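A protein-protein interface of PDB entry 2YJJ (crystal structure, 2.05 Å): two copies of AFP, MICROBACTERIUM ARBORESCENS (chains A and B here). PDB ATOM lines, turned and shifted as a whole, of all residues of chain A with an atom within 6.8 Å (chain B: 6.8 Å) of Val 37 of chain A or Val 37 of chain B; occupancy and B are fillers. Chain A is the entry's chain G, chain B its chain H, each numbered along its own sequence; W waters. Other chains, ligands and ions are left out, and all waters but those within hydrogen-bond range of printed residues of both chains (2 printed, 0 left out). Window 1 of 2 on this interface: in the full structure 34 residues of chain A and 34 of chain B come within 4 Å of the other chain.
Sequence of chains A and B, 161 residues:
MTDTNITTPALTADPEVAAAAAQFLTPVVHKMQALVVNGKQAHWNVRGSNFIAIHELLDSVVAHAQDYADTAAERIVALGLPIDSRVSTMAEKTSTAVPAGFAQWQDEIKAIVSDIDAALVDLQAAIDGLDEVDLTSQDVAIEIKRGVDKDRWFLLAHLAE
Water W1 lies within hydrogen-bond range of OG of Ser 85 of chain B (2.7 Å), O of Val 37 of chain A (3.0 Å) and NE2 of Gln 33 of chain B (3.4 Å).
Water W2 lies within hydrogen-bond range of NE2 of Gln 66 of chain B (2.9 Å) and NE2 of Gln 66 of chain A (2.9 Å).
Hydrophobic or aromatic side chains of chain A within 4 Å of the printed part of chain B: Val 36, Val 37, Trp 44, Val 87 and Met 90.
Printed residues of chain B that touch a printed residue of chain A: Gln 33, Ala 34, Val 36, Val 37, Asn 38, Lys 40, Gln 41, Trp 44, Gln 66, Ser 85, Arg 86, Val 87 and Met 90.
Hydrophobic or aromatic side chains of chain B that line the printed part of chain A: Val 36, Val 37, Trp 44, Val 87 and Met 90.
Among the printed residues, 30 pairs touch across the chains.
Among the printed residues, no Asp or Glu carboxylate lies within 4 Å of a Lys or Arg side-chain nitrogen of the other chain.
Gln 33 of chain A touches Trp 44 of chain B, and with the chains exchanged Trp 44 of chain A touches Gln 33 of chain B.
Val 37 of chain A touches Met 90 of chain B, and with the chains exchanged Met 90 of chain A touches Val 37 of chain B.
OD1 of Asn 38 of chain A is in hydrogen-bond range of N of Val 87 of chain B (3.0 Å).
The backbone NH of Ser 85 of chain B is in hydrogen-bond range of the side-chain amide oxygen of Gln 41 of chain A (2.8 Å).
The side-chain amide oxygen (OE1) of Gln 41 of chain B is in hydrogen-bond range of the backbone NH (N) of Ser 85 of chain A (2.6 Å).
OD1 of Asn 38 of chain B lies within hydrogen-bond range of N of Val 87 of chain A.
Val 37 of chain A touches five residues of chain B.
Of the printed residues of chain B, Lys 40 of chain A touches Gln 33 and Gln 66.
Of the printed residues of chain A, Gln 33 of chain B touches Val 37, Lys 40 and Trp 44.
Printed residues of chain A within 4 Å of Ala 34 of chain B: Val 87.
Of chain A, only Gln 33, Val 37, Ser 85, Val 87 and Met 90 come within 4 Å of Val 37 of chain B.
Of the printed residues of chain A, Met 90 of chain B touches Val 37, Val 87 and Met 90.
The nearest printed residue of chain A that does not touch Val 36 of chain B is Gln 33 of chain A (4.5 Å).
Among the printed residues, pairs that only touch across the chains: Val 37 of chain A with Ser 85 of chain B, Asn 38 of chain A with Arg 86 of chain B, Ser 85 of chain A with Val 37 of chain B, Gln 33 of chain A with Trp 44 of chain B, Arg 86 of chain A with Asn 38 of chain B, Trp 44 of chain A with Gln 33 of chain B, Val 37 of chain A with Val 87 of chain B, Lys 40 of chain A with Gln 66 of chain B, Trp 44 of chain A with Ser 85 of chain B, Val 87 of chain A with Val 37 of chain B, Gln 66 of chain A with Lys 40 of chain B, Val 37 of chain A with Val 37 of chain B, Val 36 of chain A with Gln 66 of chain B, Gln 41 of chain A with Arg 86 of chain B, Gln 66 of chain A with Val 36 of chain B, Met 90 of chain A with Val 87 of chain B, Arg 86 of chain A with Gln 41 of chain B, Val 37 of chain A with Gln 33 of chain B, Met 90 of chain A with Met 90 of chain B, Gln 33 of chain A with Val 37 of chain B, Met 90 of chain A with Val 37 of chain B, Val 87 of chain A with Met 90 of chain B, Ser 85 of chain A with Trp 44 of chain B, Val 37 of chain A with Met 90 of chain B, Val 87 of chain A with Ala 34 of chain B and Lys 40 of chain A with Gln 33 of chain B.
The side-chain amide oxygen (OE1) of Gln 33 of chain A lies within hydrogen-bond range of the side-chain amide nitrogen (NE2) of Gln 66 of chain A (3.2 Å).
O of Ala 34 of chain A sits at hydrogen-bond distance from ND2 of Asn 38 of chain A (3.1 Å).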
ATOM      1  N   MET A  32     -28.355  23.294 -28.974  1.00  0.00           N
ATOM      2  CA  MET A  32     -28.167  22.593 -27.713  1.00  0.00           C
ATOM      3  C   MET A  32     -26.713  22.202 -27.584  1.00  0.00           C
ATOM      4  O   MET A  32     -26.107  22.423 -26.517  1.00  0.00           O
ATOM      5  CB  MET A  32     -29.122  21.394 -27.528  1.00  0.00           C
ATOM      6  CG  MET A  32     -30.594  21.876 -27.353  1.00  0.00           C
ATOM      7  SD  MET A  32     -30.868  22.915 -25.833  1.00  0.00           S
ATOM      8  CE  MET A  32     -30.946  24.478 -26.461  1.00  0.00           C
ATOM      9  N   GLN A  33     -26.147  21.671 -28.673  1.00  0.00           N
ATOM     10  CA  GLN A  33     -24.771  21.182 -28.653  1.00  0.00           C
ATOM     11  C   GLN A  33     -23.811  22.382 -28.427  1.00  0.00           C
ATOM     12  O   GLN A  33     -22.839  22.255 -27.710  1.00  0.00           O
ATOM     13  CB  GLN A  33     -24.415  20.375 -29.922  1.00  0.00           C
ATOM     14  CG  GLN A  33     -23.025  19.645 -29.880  1.00  0.00           C
ATOM     15  CD  GLN A  33     -22.966  18.640 -28.724  1.00  0.00           C
ATOM     16  OE1 GLN A  33     -22.351  18.916 -27.680  1.00  0.00           O
ATOM     17  NE2 GLN A  33     -23.642  17.518 -28.868  1.00  0.00           N
ATOM     18  N   ALA A  34     -24.101  23.535 -29.043  1.00  0.00           N
ATOM     19  CA  ALA A  34     -23.332  24.735 -28.879  1.00  0.00           C
ATOM     20  C   ALA A  34     -23.434  25.251 -27.425  1.00  0.00           C
ATOM     21  O   ALA A  34     -22.459  25.738 -26.857  1.00  0.00           O
ATOM     22  CB  ALA A  34     -23.849  25.868 -29.862  1.00  0.00           C
ATOM     23  N   LEU A  35     -24.633  25.178 -26.840  1.00  0.00           N
ATOM     24  CA  LEU A  35     -24.807  25.504 -25.433  1.00  0.00           C
ATOM     25  C   LEU A  35     -23.907  24.670 -24.495  1.00  0.00           C
ATOM     26  O   LEU A  35     -23.412  25.182 -23.502  1.00  0.00           O
ATOM     27  CB  LEU A  35     -26.287  25.454 -25.007  1.00  0.00           C
ATOM     28  CG  LEU A  35     -26.572  25.963 -23.573  1.00  0.00           C
ATOM     29  CD1 LEU A  35     -26.146  27.423 -23.434  1.00  0.00           C
ATOM     30  CD2 LEU A  35     -28.055  25.863 -23.260  1.00  0.00           C
ATOM     31  N   VAL A  36     -23.711  23.395 -24.793  1.00  0.00           N
ATOM     32  CA  VAL A  36     -22.749  22.537 -23.999  1.00  0.00           C
ATOM     33  C   VAL A  36     -21.329  23.176 -24.031  1.00  0.00           C
ATOM     34  O   VAL A  36     -20.667  23.315 -23.008  1.00  0.00           O
ATOM     35  CB  VAL A  36     -22.660  21.122 -24.557  1.00  0.00           C
ATOM     36  CG1 VAL A  36     -21.507  20.292 -23.862  1.00  0.00           C
ATOM     37  CG2 VAL A  36     -24.059  20.453 -24.439  1.00  0.00           C
ATOM     38  N   VAL A  37     -20.873  23.584 -25.206  1.00  0.00           N
ATOM     39  CA  VAL A  37     -19.493  24.055 -25.348  1.00  0.00           C
ATOM     40  C   VAL A  37     -19.354  25.437 -24.750  1.00  0.00           C
ATOM     41  O   VAL A  37     -18.497  25.683 -23.887  1.00  0.00           O
ATOM     42  CB  VAL A  37     -19.105  24.076 -26.846  1.00  0.00           C
ATOM     43  CG1 VAL A  37     -17.795  24.815 -27.020  1.00  0.00           C
ATOM     44  CG2 VAL A  37     -18.997  22.560 -27.343  1.00  0.00           C
ATOM     45  N   ASN A  38     -20.298  26.303 -25.084  1.00  0.00           N
ATOM     46  CA  ASN A  38     -20.255  27.675 -24.585  1.00  0.00           C
ATOM     47  C   ASN A  38     -20.651  27.776 -23.098  1.00  0.00           C
ATOM     48  O   ASN A  38     -20.221  28.692 -22.390  1.00  0.00           O
ATOM     49  CB  ASN A  38     -21.147  28.610 -25.447  1.00  0.00           C
ATOM     50  CG  ASN A  38     -20.666  28.682 -26.897  1.00  0.00           C
ATOM     51  OD1 ASN A  38     -19.456  28.795 -27.159  1.00  0.00           O
ATOM     52  ND2 ASN A  38     -21.609  28.508 -27.858  1.00  0.00           N
ATOM     53  N   GLY A  39     -21.516  26.898 -22.636  1.00  0.00           N
ATOM     54  CA  GLY A  39     -21.805  26.708 -21.199  1.00  0.00           C
ATOM     55  C   GLY A  39     -20.550  26.337 -20.385  1.00  0.00           C
ATOM     56  O   GLY A  39     -20.370  26.812 -19.262  1.00  0.00           O
ATOM     57  N   LYS A  40     -19.724  25.446 -20.924  1.00  0.00           N
ATOM     58  CA  LYS A  40     -18.489  25.057 -20.257  1.00  0.00           C
ATOM     59  C   LYS A  40     -17.551  26.273 -20.239  1.00  0.00           C
ATOM     60  O   LYS A  40     -16.884  26.500 -19.259  1.00  0.00           O
ATOM     61  CB  LYS A  40     -17.788  23.894 -20.981  1.00  0.00           C
ATOM     62  CG  LYS A  40     -18.481  22.488 -20.733  1.00  0.00           C
ATOM     63  CD  LYS A  40     -18.355  22.071 -19.222  1.00  0.00           C
ATOM     64  CE  LYS A  40     -18.573  20.599 -18.902  1.00  0.00           C
ATOM     65  NZ  LYS A  40     -18.167  20.505 -17.420  1.00  0.00           N
ATOM     66  N   GLN A  41     -17.485  27.019 -21.321  1.00  0.00           N
ATOM     67  CA  GLN A  41     -16.633  28.188 -21.347  1.00  0.00           C
ATOM     68  C   GLN A  41     -17.010  29.174 -20.207  1.00  0.00           C
ATOM     69  O   GLN A  41     -16.156  29.714 -19.510  1.00  0.00           O
ATOM     70  CB  GLN A  41     -16.739  28.860 -22.738  1.00  0.00           C
ATOM     71  CG  GLN A  41     -16.370  30.327 -22.782  1.00  0.00           C
ATOM     72  CD  GLN A  41     -14.861  30.433 -22.876  1.00  0.00           C
ATOM     73  OE1 GLN A  41     -14.169  29.390 -22.866  1.00  0.00           O
ATOM     74  NE2 GLN A  41     -14.326  31.653 -22.979  1.00  0.00           N
ATOM     75  N   ALA A  42     -18.301  29.419 -20.037  1.00  0.00           N
ATOM     76  CA  ALA A  42     -18.799  30.287 -18.955  1.00  0.00           C
ATOM     77  C   ALA A  42     -18.537  29.662 -17.571  1.00  0.00           C
ATOM     78  O   ALA A  42     -18.079  30.281 -16.654  1.00  0.00           O
ATOM     79  CB  ALA A  42     -20.308  30.536 -19.176  1.00  0.00           C
ATOM     80  N   TRP A  44     -16.050  27.618 -16.755  1.00  0.00           N
ATOM     81  CA  TRP A  44     -14.619  27.778 -16.488  1.00  0.00           C
ATOM     82  C   TRP A  44     -14.197  29.205 -16.085  1.00  0.00           C
ATOM     83  O   TRP A  44     -13.309  29.384 -15.240  1.00  0.00           O
ATOM     84  CB  TRP A  44     -13.758  27.323 -17.716  1.00  0.00           C
ATOM     85  CG  TRP A  44     -13.918  25.806 -17.942  1.00  0.00           C
ATOM     86  CD1 TRP A  44     -14.149  24.858 -16.975  1.00  0.00           C
ATOM     87  CD2 TRP A  44     -13.935  25.119 -19.202  1.00  0.00           C
ATOM     88  NE1 TRP A  44     -14.324  23.610 -17.563  1.00  0.00           N
ATOM     89  CE2 TRP A  44     -14.165  23.743 -18.927  1.00  0.00           C
ATOM     90  CE3 TRP A  44     -13.734  25.530 -20.554  1.00  0.00           C
ATOM     91  CZ2 TRP A  44     -14.215  22.751 -19.963  1.00  0.00           C
ATOM     92  CZ3 TRP A  44     -13.775  24.555 -21.564  1.00  0.00           C
ATOM     93  CH2 TRP A  44     -14.035  23.181 -21.263  1.00  0.00           C
ATOM     94  N   VAL A  62     -25.353  22.903 -18.744  1.00  0.00           N
ATOM     95  CA  VAL A  62     -24.573  22.147 -19.708  1.00  0.00           C
ATOM     96  C   VAL A  62     -25.030  20.671 -19.790  1.00  0.00           C
ATOM     97  O   VAL A  62     -25.193  20.182 -20.858  1.00  0.00           O
ATOM     98  CB  VAL A  62     -23.078  22.226 -19.396  1.00  0.00           C
ATOM     99  CG1 VAL A  62     -22.271  21.130 -20.081  1.00  0.00           C
ATOM    100  CG2 VAL A  62     -22.551  23.636 -19.682  1.00  0.00           C
ATOM    101  N   GLN A  66     -26.725  18.855 -23.103  1.00  0.00           N
ATOM    102  CA  GLN A  66     -26.136  17.668 -23.756  1.00  0.00           C
ATOM    103  C   GLN A  66     -27.208  16.605 -23.960  1.00  0.00           C
ATOM    104  O   GLN A  66     -27.239  15.919 -25.021  1.00  0.00           O
ATOM    105  CB  GLN A  66     -25.013  17.010 -22.917  1.00  0.00           C
ATOM    106  CG  GLN A  66     -24.242  15.902 -23.672  1.00  0.00           C
ATOM    107  CD  GLN A  66     -23.796  16.359 -25.122  1.00  0.00           C
ATOM    108  OE1 GLN A  66     -24.517  16.174 -26.100  1.00  0.00           O
ATOM    109  NE2 GLN A  66     -22.619  16.923 -25.230  1.00  0.00           N
ATOM    110  N   SER A  85     -23.802  17.255 -37.219  1.00  0.00           N
ATOM    111  CA  SER A  85     -23.437  18.184 -36.119  1.00  0.00           C
ATOM    112  C   SER A  85     -21.906  18.205 -35.861  1.00  0.00           C
ATOM    113  O   SER A  85     -21.473  18.293 -34.714  1.00  0.00           O
ATOM    114  CB  SER A  85     -24.186  17.827 -34.813  1.00  0.00           C
ATOM    115  OG  SER A  85     -24.007  18.896 -33.798  1.00  0.00           O
ATOM    116  N   ARG A  86     -21.091  18.101 -36.896  1.00  0.00           N
ATOM    117  CA  ARG A  86     -19.653  18.180 -36.710  1.00  0.00           C
ATOM    118  C   ARG A  86     -19.319  19.605 -36.156  1.00  0.00           C
ATOM    119  O   ARG A  86     -20.109  20.512 -36.332  1.00  0.00           O
ATOM    120  CB  ARG A  86     -18.960  17.995 -38.061  1.00  0.00           C
ATOM    121  CG  ARG A  86     -19.024  16.599 -38.701  1.00  0.00           C
ATOM    122  CD  ARG A  86     -18.370  16.668 -40.082  1.00  0.00           C
ATOM    123  NE  ARG A  86     -19.212  17.521 -40.946  1.00  0.00           N
ATOM    124  CZ  ARG A  86     -18.899  17.878 -42.199  1.00  0.00           C
ATOM    125  NH1 ARG A  86     -17.755  17.502 -42.765  1.00  0.00           N
ATOM    126  NH2 ARG A  86     -19.737  18.595 -42.886  1.00  0.00           N
ATOM    127  N   VAL A  87     -18.162  19.789 -35.541  1.00  0.00           N
ATOM    128  CA  VAL A  87     -17.791  21.126 -34.958  1.00  0.00           C
ATOM    129  C   VAL A  87     -17.895  22.248 -36.036  1.00  0.00           C
ATOM    130  O   VAL A  87     -18.405  23.340 -35.755  1.00  0.00           O
ATOM    131  CB  VAL A  87     -16.353  21.069 -34.379  1.00  0.00           C
ATOM    132  CG1 VAL A  87     -15.767  22.510 -34.131  1.00  0.00           C
ATOM    133  CG2 VAL A  87     -16.379  20.333 -33.002  1.00  0.00           C
ATOM    134  N   SER A  88     -17.399  21.957 -37.256  1.00  0.00           N
ATOM    135  CA  SER A  88     -17.357  22.970 -38.342  1.00  0.00           C
ATOM    136  C   SER A  88     -18.800  23.404 -38.686  1.00  0.00           C
ATOM    137  O   SER A  88     -19.085  24.579 -38.830  1.00  0.00           O
ATOM    138  CB  SER A  88     -16.651  22.440 -39.640  1.00  0.00           C
ATOM    139  OG  SER A  88     -17.050  21.091 -39.946  1.00  0.00           O
ATOM    140  N   MET A  90     -21.693  23.091 -36.770  1.00  0.00           N
ATOM    141  CA  MET A  90     -22.294  23.720 -35.607  1.00  0.00           C
ATOM    142  C   MET A  90     -21.753  25.179 -35.486  1.00  0.00           C
ATOM    143  O   MET A  90     -22.488  26.093 -35.163  1.00  0.00           O
ATOM    144  CB  MET A  90     -21.986  22.824 -34.356  1.00  0.00           C
ATOM    145  CG  MET A  90     -22.385  23.489 -33.027  1.00  0.00           C
ATOM    146  SD  MET A  90     -21.860  22.537 -31.609  1.00  0.00           S
ATOM    147  CE  MET A  90     -20.092  22.914 -31.578  1.00  0.00           C
ATOM    148  N   MET B  32     -10.007  17.978 -26.892  1.00  0.00           N
ATOM    149  CA  MET B  32     -10.907  17.158 -26.098  1.00  0.00           C
ATOM    150  C   MET B  32     -12.393  17.636 -26.256  1.00  0.00           C
ATOM    151  O   MET B  32     -13.314  16.802 -26.377  1.00  0.00           O
ATOM    152  CB  MET B  32     -10.516  17.079 -24.632  1.00  0.00           C
ATOM    153  CG  MET B  32      -9.229  16.341 -24.289  1.00  0.00           C
ATOM    154  SD  MET B  32      -9.296  14.555 -24.849  1.00  0.00           S
ATOM    155  CE  MET B  32      -8.217  14.621 -26.172  1.00  0.00           C
ATOM    156  N   GLN B  33     -12.626  18.955 -26.221  1.00  0.00           N
ATOM    157  CA  GLN B  33     -13.991  19.457 -26.324  1.00  0.00           C
ATOM    158  C   GLN B  33     -14.495  19.178 -27.720  1.00  0.00           C
ATOM    159  O   GLN B  33     -15.721  18.966 -27.902  1.00  0.00           O
ATOM    160  CB  GLN B  33     -14.087  21.004 -26.022  1.00  0.00           C
ATOM    161  CG  GLN B  33     -15.549  21.563 -25.910  1.00  0.00           C
ATOM    162  CD  GLN B  33     -16.314  20.916 -24.739  1.00  0.00           C
ATOM    163  OE1 GLN B  33     -17.182  20.036 -24.942  1.00  0.00           O
ATOM    164  NE2 GLN B  33     -15.922  21.259 -23.531  1.00  0.00           N
ATOM    165  N   ALA B  34     -13.627  19.282 -28.731  1.00  0.00           N
ATOM    166  CA  ALA B  34     -14.069  18.929 -30.098  1.00  0.00           C
ATOM    167  C   ALA B  34     -14.431  17.464 -30.181  1.00  0.00           C
ATOM    168  O   ALA B  34     -15.360  17.056 -30.890  1.00  0.00           O
ATOM    169  CB  ALA B  34     -12.942  19.256 -31.244  1.00  0.00           C
ATOM    170  N   LEU B  35     -13.663  16.638 -29.497  1.00  0.00           N
ATOM    171  CA  LEU B  35     -13.904  15.208 -29.524  1.00  0.00           C
ATOM    172  C   LEU B  35     -15.271  14.847 -28.914  1.00  0.00           C
ATOM    173  O   LEU B  35     -15.883  13.812 -29.238  1.00  0.00           O
ATOM    174  CB  LEU B  35     -12.778  14.468 -28.813  1.00  0.00           C
ATOM    175  CG  LEU B  35     -12.866  12.967 -28.644  1.00  0.00           C
ATOM    176  CD1 LEU B  35     -13.261  12.356 -29.969  1.00  0.00           C
ATOM    177  CD2 LEU B  35     -11.507  12.346 -28.091  1.00  0.00           C
ATOM    178  N   VAL B  36     -15.742  15.669 -28.000  1.00  0.00           N
ATOM    179  CA  VAL B  36     -17.067  15.456 -27.411  1.00  0.00           C
ATOM    180  C   VAL B  36     -18.066  15.625 -28.576  1.00  0.00           C
ATOM    181  O   VAL B  36     -18.999  14.860 -28.717  1.00  0.00           O
ATOM    182  CB  VAL B  36     -17.338  16.555 -26.315  1.00  0.00           C
ATOM    183  CG1 VAL B  36     -18.879  16.662 -25.957  1.00  0.00           C
ATOM    184  CG2 VAL B  36     -16.402  16.306 -25.018  1.00  0.00           C
ATOM    185  N   VAL B  37     -17.889  16.691 -29.371  1.00  0.00           N
ATOM    186  CA  VAL B  37     -18.934  17.137 -30.351  1.00  0.00           C
ATOM    187  C   VAL B  37     -18.865  16.192 -31.521  1.00  0.00           C
ATOM    188  O   VAL B  37     -19.877  15.600 -31.904  1.00  0.00           O
ATOM    189  CB  VAL B  37     -18.754  18.622 -30.768  1.00  0.00           C
ATOM    190  CG1 VAL B  37     -19.743  19.050 -31.874  1.00  0.00           C
ATOM    191  CG2 VAL B  37     -18.908  19.543 -29.540  1.00  0.00           C
ATOM    192  N   ASN B  38     -17.672  15.974 -32.039  1.00  0.00           N
ATOM    193  CA  ASN B  38     -17.475  15.030 -33.151  1.00  0.00           C
ATOM    194  C   ASN B  38     -17.721  13.543 -32.787  1.00  0.00           C
ATOM    195  O   ASN B  38     -18.112  12.811 -33.630  1.00  0.00           O
ATOM    196  CB  ASN B  38     -16.075  15.243 -33.802  1.00  0.00           C
ATOM    197  CG  ASN B  38     -15.919  16.641 -34.306  1.00  0.00           C
ATOM    198  OD1 ASN B  38     -16.880  17.186 -34.833  1.00  0.00           O
ATOM    199  ND2 ASN B  38     -14.741  17.278 -34.082  1.00  0.00           N
ATOM    200  N   GLY B  39     -17.391  13.110 -31.566  1.00  0.00           N
ATOM    201  CA  GLY B  39     -17.727  11.801 -31.059  1.00  0.00           C
ATOM    202  C   GLY B  39     -19.239  11.646 -30.914  1.00  0.00           C
ATOM    203  O   GLY B  39     -19.742  10.571 -31.117  1.00  0.00           O
ATOM    204  N   LYS B  40     -19.939  12.686 -30.483  1.00  0.00           N
ATOM    205  CA  LYS B  40     -21.401  12.665 -30.479  1.00  0.00           C
ATOM    206  C   LYS B  40     -21.888  12.480 -31.919  1.00  0.00           C
ATOM    207  O   LYS B  40     -22.800  11.680 -32.121  1.00  0.00           O
ATOM    208  CB  LYS B  40     -22.053  13.901 -29.828  1.00  0.00           C
ATOM    209  CG  LYS B  40     -22.147  13.830 -28.309  1.00  0.00           C
ATOM    210  CD  LYS B  40     -23.022  12.647 -27.792  1.00  0.00           C
ATOM    211  CE  LYS B  40     -23.267  12.700 -26.273  1.00  0.00           C
ATOM    212  NZ  LYS B  40     -24.181  11.576 -25.891  1.00  0.00           N
ATOM    213  N   GLN B  41     -21.282  13.195 -32.881  1.00  0.00           N
ATOM    214  CA  GLN B  41     -21.688  13.071 -34.301  1.00  0.00           C
ATOM    215  C   GLN B  41     -21.530  11.572 -34.750  1.00  0.00           C
ATOM    216  O   GLN B  41     -22.359  10.998 -35.414  1.00  0.00           O
ATOM    217  CB  GLN B  41     -20.776  14.014 -35.161  1.00  0.00           C
ATOM    218  CG  GLN B  41     -20.875  13.800 -36.670  1.00  0.00           C
ATOM    219  CD  GLN B  41     -22.141  14.250 -37.323  1.00  0.00           C
ATOM    220  OE1 GLN B  41     -23.006  14.789 -36.672  1.00  0.00           O
ATOM    221  NE2 GLN B  41     -22.247  14.053 -38.653  1.00  0.00           N
ATOM    222  N   ALA B  42     -20.413  10.964 -34.377  1.00  0.00           N
ATOM    223  CA  ALA B  42     -20.112   9.578 -34.789  1.00  0.00           C
ATOM    224  C   ALA B  42     -21.142   8.624 -34.107  1.00  0.00           C
ATOM    225  O   ALA B  42     -21.704   7.698 -34.724  1.00  0.00           O
ATOM    226  CB  ALA B  42     -18.647   9.231 -34.336  1.00  0.00           C
ATOM    227  N   TRP B  44     -24.238   9.300 -33.135  1.00  0.00           N
ATOM    228  CA  TRP B  44     -25.594   9.402 -33.730  1.00  0.00           C
ATOM    229  C   TRP B  44     -25.675   8.690 -35.071  1.00  0.00           C
ATOM    230  O   TRP B  44     -26.701   8.119 -35.421  1.00  0.00           O
ATOM    231  CB  TRP B  44     -26.029  10.892 -33.885  1.00  0.00           C
ATOM    232  CG  TRP B  44     -26.134  11.518 -32.481  1.00  0.00           C
ATOM    233  CD1 TRP B  44     -26.530  10.872 -31.305  1.00  0.00           C
ATOM    234  CD2 TRP B  44     -25.848  12.864 -32.104  1.00  0.00           C
ATOM    235  NE1 TRP B  44     -26.593  11.771 -30.258  1.00  0.00           N
ATOM    236  CE2 TRP B  44     -26.143  12.984 -30.706  1.00  0.00           C
ATOM    237  CE3 TRP B  44     -25.412  14.009 -32.819  1.00  0.00           C
ATOM    238  CZ2 TRP B  44     -25.991  14.197 -30.000  1.00  0.00           C
ATOM    239  CZ3 TRP B  44     -25.286  15.198 -32.129  1.00  0.00           C
ATOM    240  CH2 TRP B  44     -25.547  15.288 -30.735  1.00  0.00           C
ATOM    241  N   VAL B  62     -16.737   9.945 -25.470  1.00  0.00           N
ATOM    242  CA  VAL B  62     -17.265  11.273 -25.377  1.00  0.00           C
ATOM    243  C   VAL B  62     -17.297  11.712 -23.891  1.00  0.00           C
ATOM    244  O   VAL B  62     -16.946  12.829 -23.615  1.00  0.00           O
ATOM    245  CB  VAL B  62     -18.689  11.351 -26.030  1.00  0.00           C
ATOM    246  CG1 VAL B  62     -19.473  12.613 -25.588  1.00  0.00           C
ATOM    247  CG2 VAL B  62     -18.537  11.360 -27.583  1.00  0.00           C
ATOM    248  N   GLN B  66     -15.015  14.785 -22.336  1.00  0.00           N
ATOM    249  CA  GLN B  66     -15.593  15.896 -21.626  1.00  0.00           C
ATOM    250  C   GLN B  66     -14.899  16.074 -20.274  1.00  0.00           C
ATOM    251  O   GLN B  66     -14.547  17.192 -19.901  1.00  0.00           O
ATOM    252  CB  GLN B  66     -17.130  15.742 -21.466  1.00  0.00           C
ATOM    253  CG  GLN B  66     -17.818  17.026 -20.872  1.00  0.00           C
ATOM    254  CD  GLN B  66     -17.567  18.295 -21.783  1.00  0.00           C
ATOM    255  OE1 GLN B  66     -16.618  19.104 -21.561  1.00  0.00           O
ATOM    256  NE2 GLN B  66     -18.405  18.458 -22.784  1.00  0.00           N
ATOM    257  N   SER B  85     -12.577  28.833 -25.107  1.00  0.00           N
ATOM    258  CA  SER B  85     -13.031  27.610 -25.646  1.00  0.00           C
ATOM    259  C   SER B  85     -14.494  27.785 -26.133  1.00  0.00           C
ATOM    260  O   SER B  85     -15.270  26.824 -26.170  1.00  0.00           O
ATOM    261  CB  SER B  85     -12.920  26.522 -24.556  1.00  0.00           C
ATOM    262  OG  SER B  85     -13.256  25.257 -25.112  1.00  0.00           O
ATOM    263  N   ARG B  86     -14.859  28.989 -26.544  1.00  0.00           N
ATOM    264  CA  ARG B  86     -16.087  29.188 -27.275  1.00  0.00           C
ATOM    265  C   ARG B  86     -16.123  28.364 -28.601  1.00  0.00           C
ATOM    266  O   ARG B  86     -15.078  28.011 -29.174  1.00  0.00           O
ATOM    267  CB  ARG B  86     -16.241  30.653 -27.644  1.00  0.00           C
ATOM    268  CG  ARG B  86     -16.176  31.626 -26.507  1.00  0.00           C
ATOM    269  CD  ARG B  86     -16.264  33.001 -27.065  1.00  0.00           C
ATOM    270  NE  ARG B  86     -14.970  33.362 -27.617  1.00  0.00           N
ATOM    271  CZ  ARG B  86     -14.743  34.426 -28.380  1.00  0.00           C
ATOM    272  NH1 ARG B  86     -15.729  35.260 -28.668  1.00  0.00           N
ATOM    273  NH2 ARG B  86     -13.501  34.657 -28.833  1.00  0.00           N
ATOM    274  N   VAL B  87     -17.328  28.072 -29.098  1.00  0.00           N
ATOM    275  CA  VAL B  87     -17.448  27.206 -30.284  1.00  0.00           C
ATOM    276  C   VAL B  87     -16.640  27.753 -31.491  1.00  0.00           C
ATOM    277  O   VAL B  87     -15.970  26.972 -32.176  1.00  0.00           O
ATOM    278  CB  VAL B  87     -18.907  27.124 -30.699  1.00  0.00           C
ATOM    279  CG1 VAL B  87     -19.071  26.590 -32.216  1.00  0.00           C
ATOM    280  CG2 VAL B  87     -19.673  26.235 -29.713  1.00  0.00           C
ATOM    281  N   SER B  88     -16.775  29.060 -31.791  1.00  0.00           N
ATOM    282  CA  SER B  88     -16.040  29.715 -32.913  1.00  0.00           C
ATOM    283  C   SER B  88     -14.535  29.517 -32.742  1.00  0.00           C
ATOM    284  O   SER B  88     -13.864  29.095 -33.665  1.00  0.00           O
ATOM    285  CB  SER B  88     -16.353  31.218 -33.012  1.00  0.00           C
ATOM    286  OG  SER B  88     -16.020  31.821 -31.757  1.00  0.00           O
ATOM    287  N   MET B  90     -12.924  27.098 -30.839  1.00  0.00           N
ATOM    288  CA  MET B  90     -12.703  25.667 -31.016  1.00  0.00           C
ATOM    289  C   MET B  90     -12.736  25.241 -32.479  1.00  0.00           C
ATOM    290  O   MET B  90     -11.884  24.437 -32.924  1.00  0.00           O
ATOM    291  CB  MET B  90     -13.687  24.858 -30.147  1.00  0.00           C
ATOM    292  CG  MET B  90     -13.612  23.388 -30.329  1.00  0.00           C
ATOM    293  SD  MET B  90     -14.971  22.552 -29.448  1.00  0.00           S
ATOM    294  CE  MET B  90     -16.436  23.242 -30.362  1.00  0.00           C
HETATM  295  O   HOH W   1     -15.738  24.571 -24.211  1.00  0.00           O
HETATM  296  O   HOH W   2     -20.858  16.954 -22.908  1.00  0.00           O
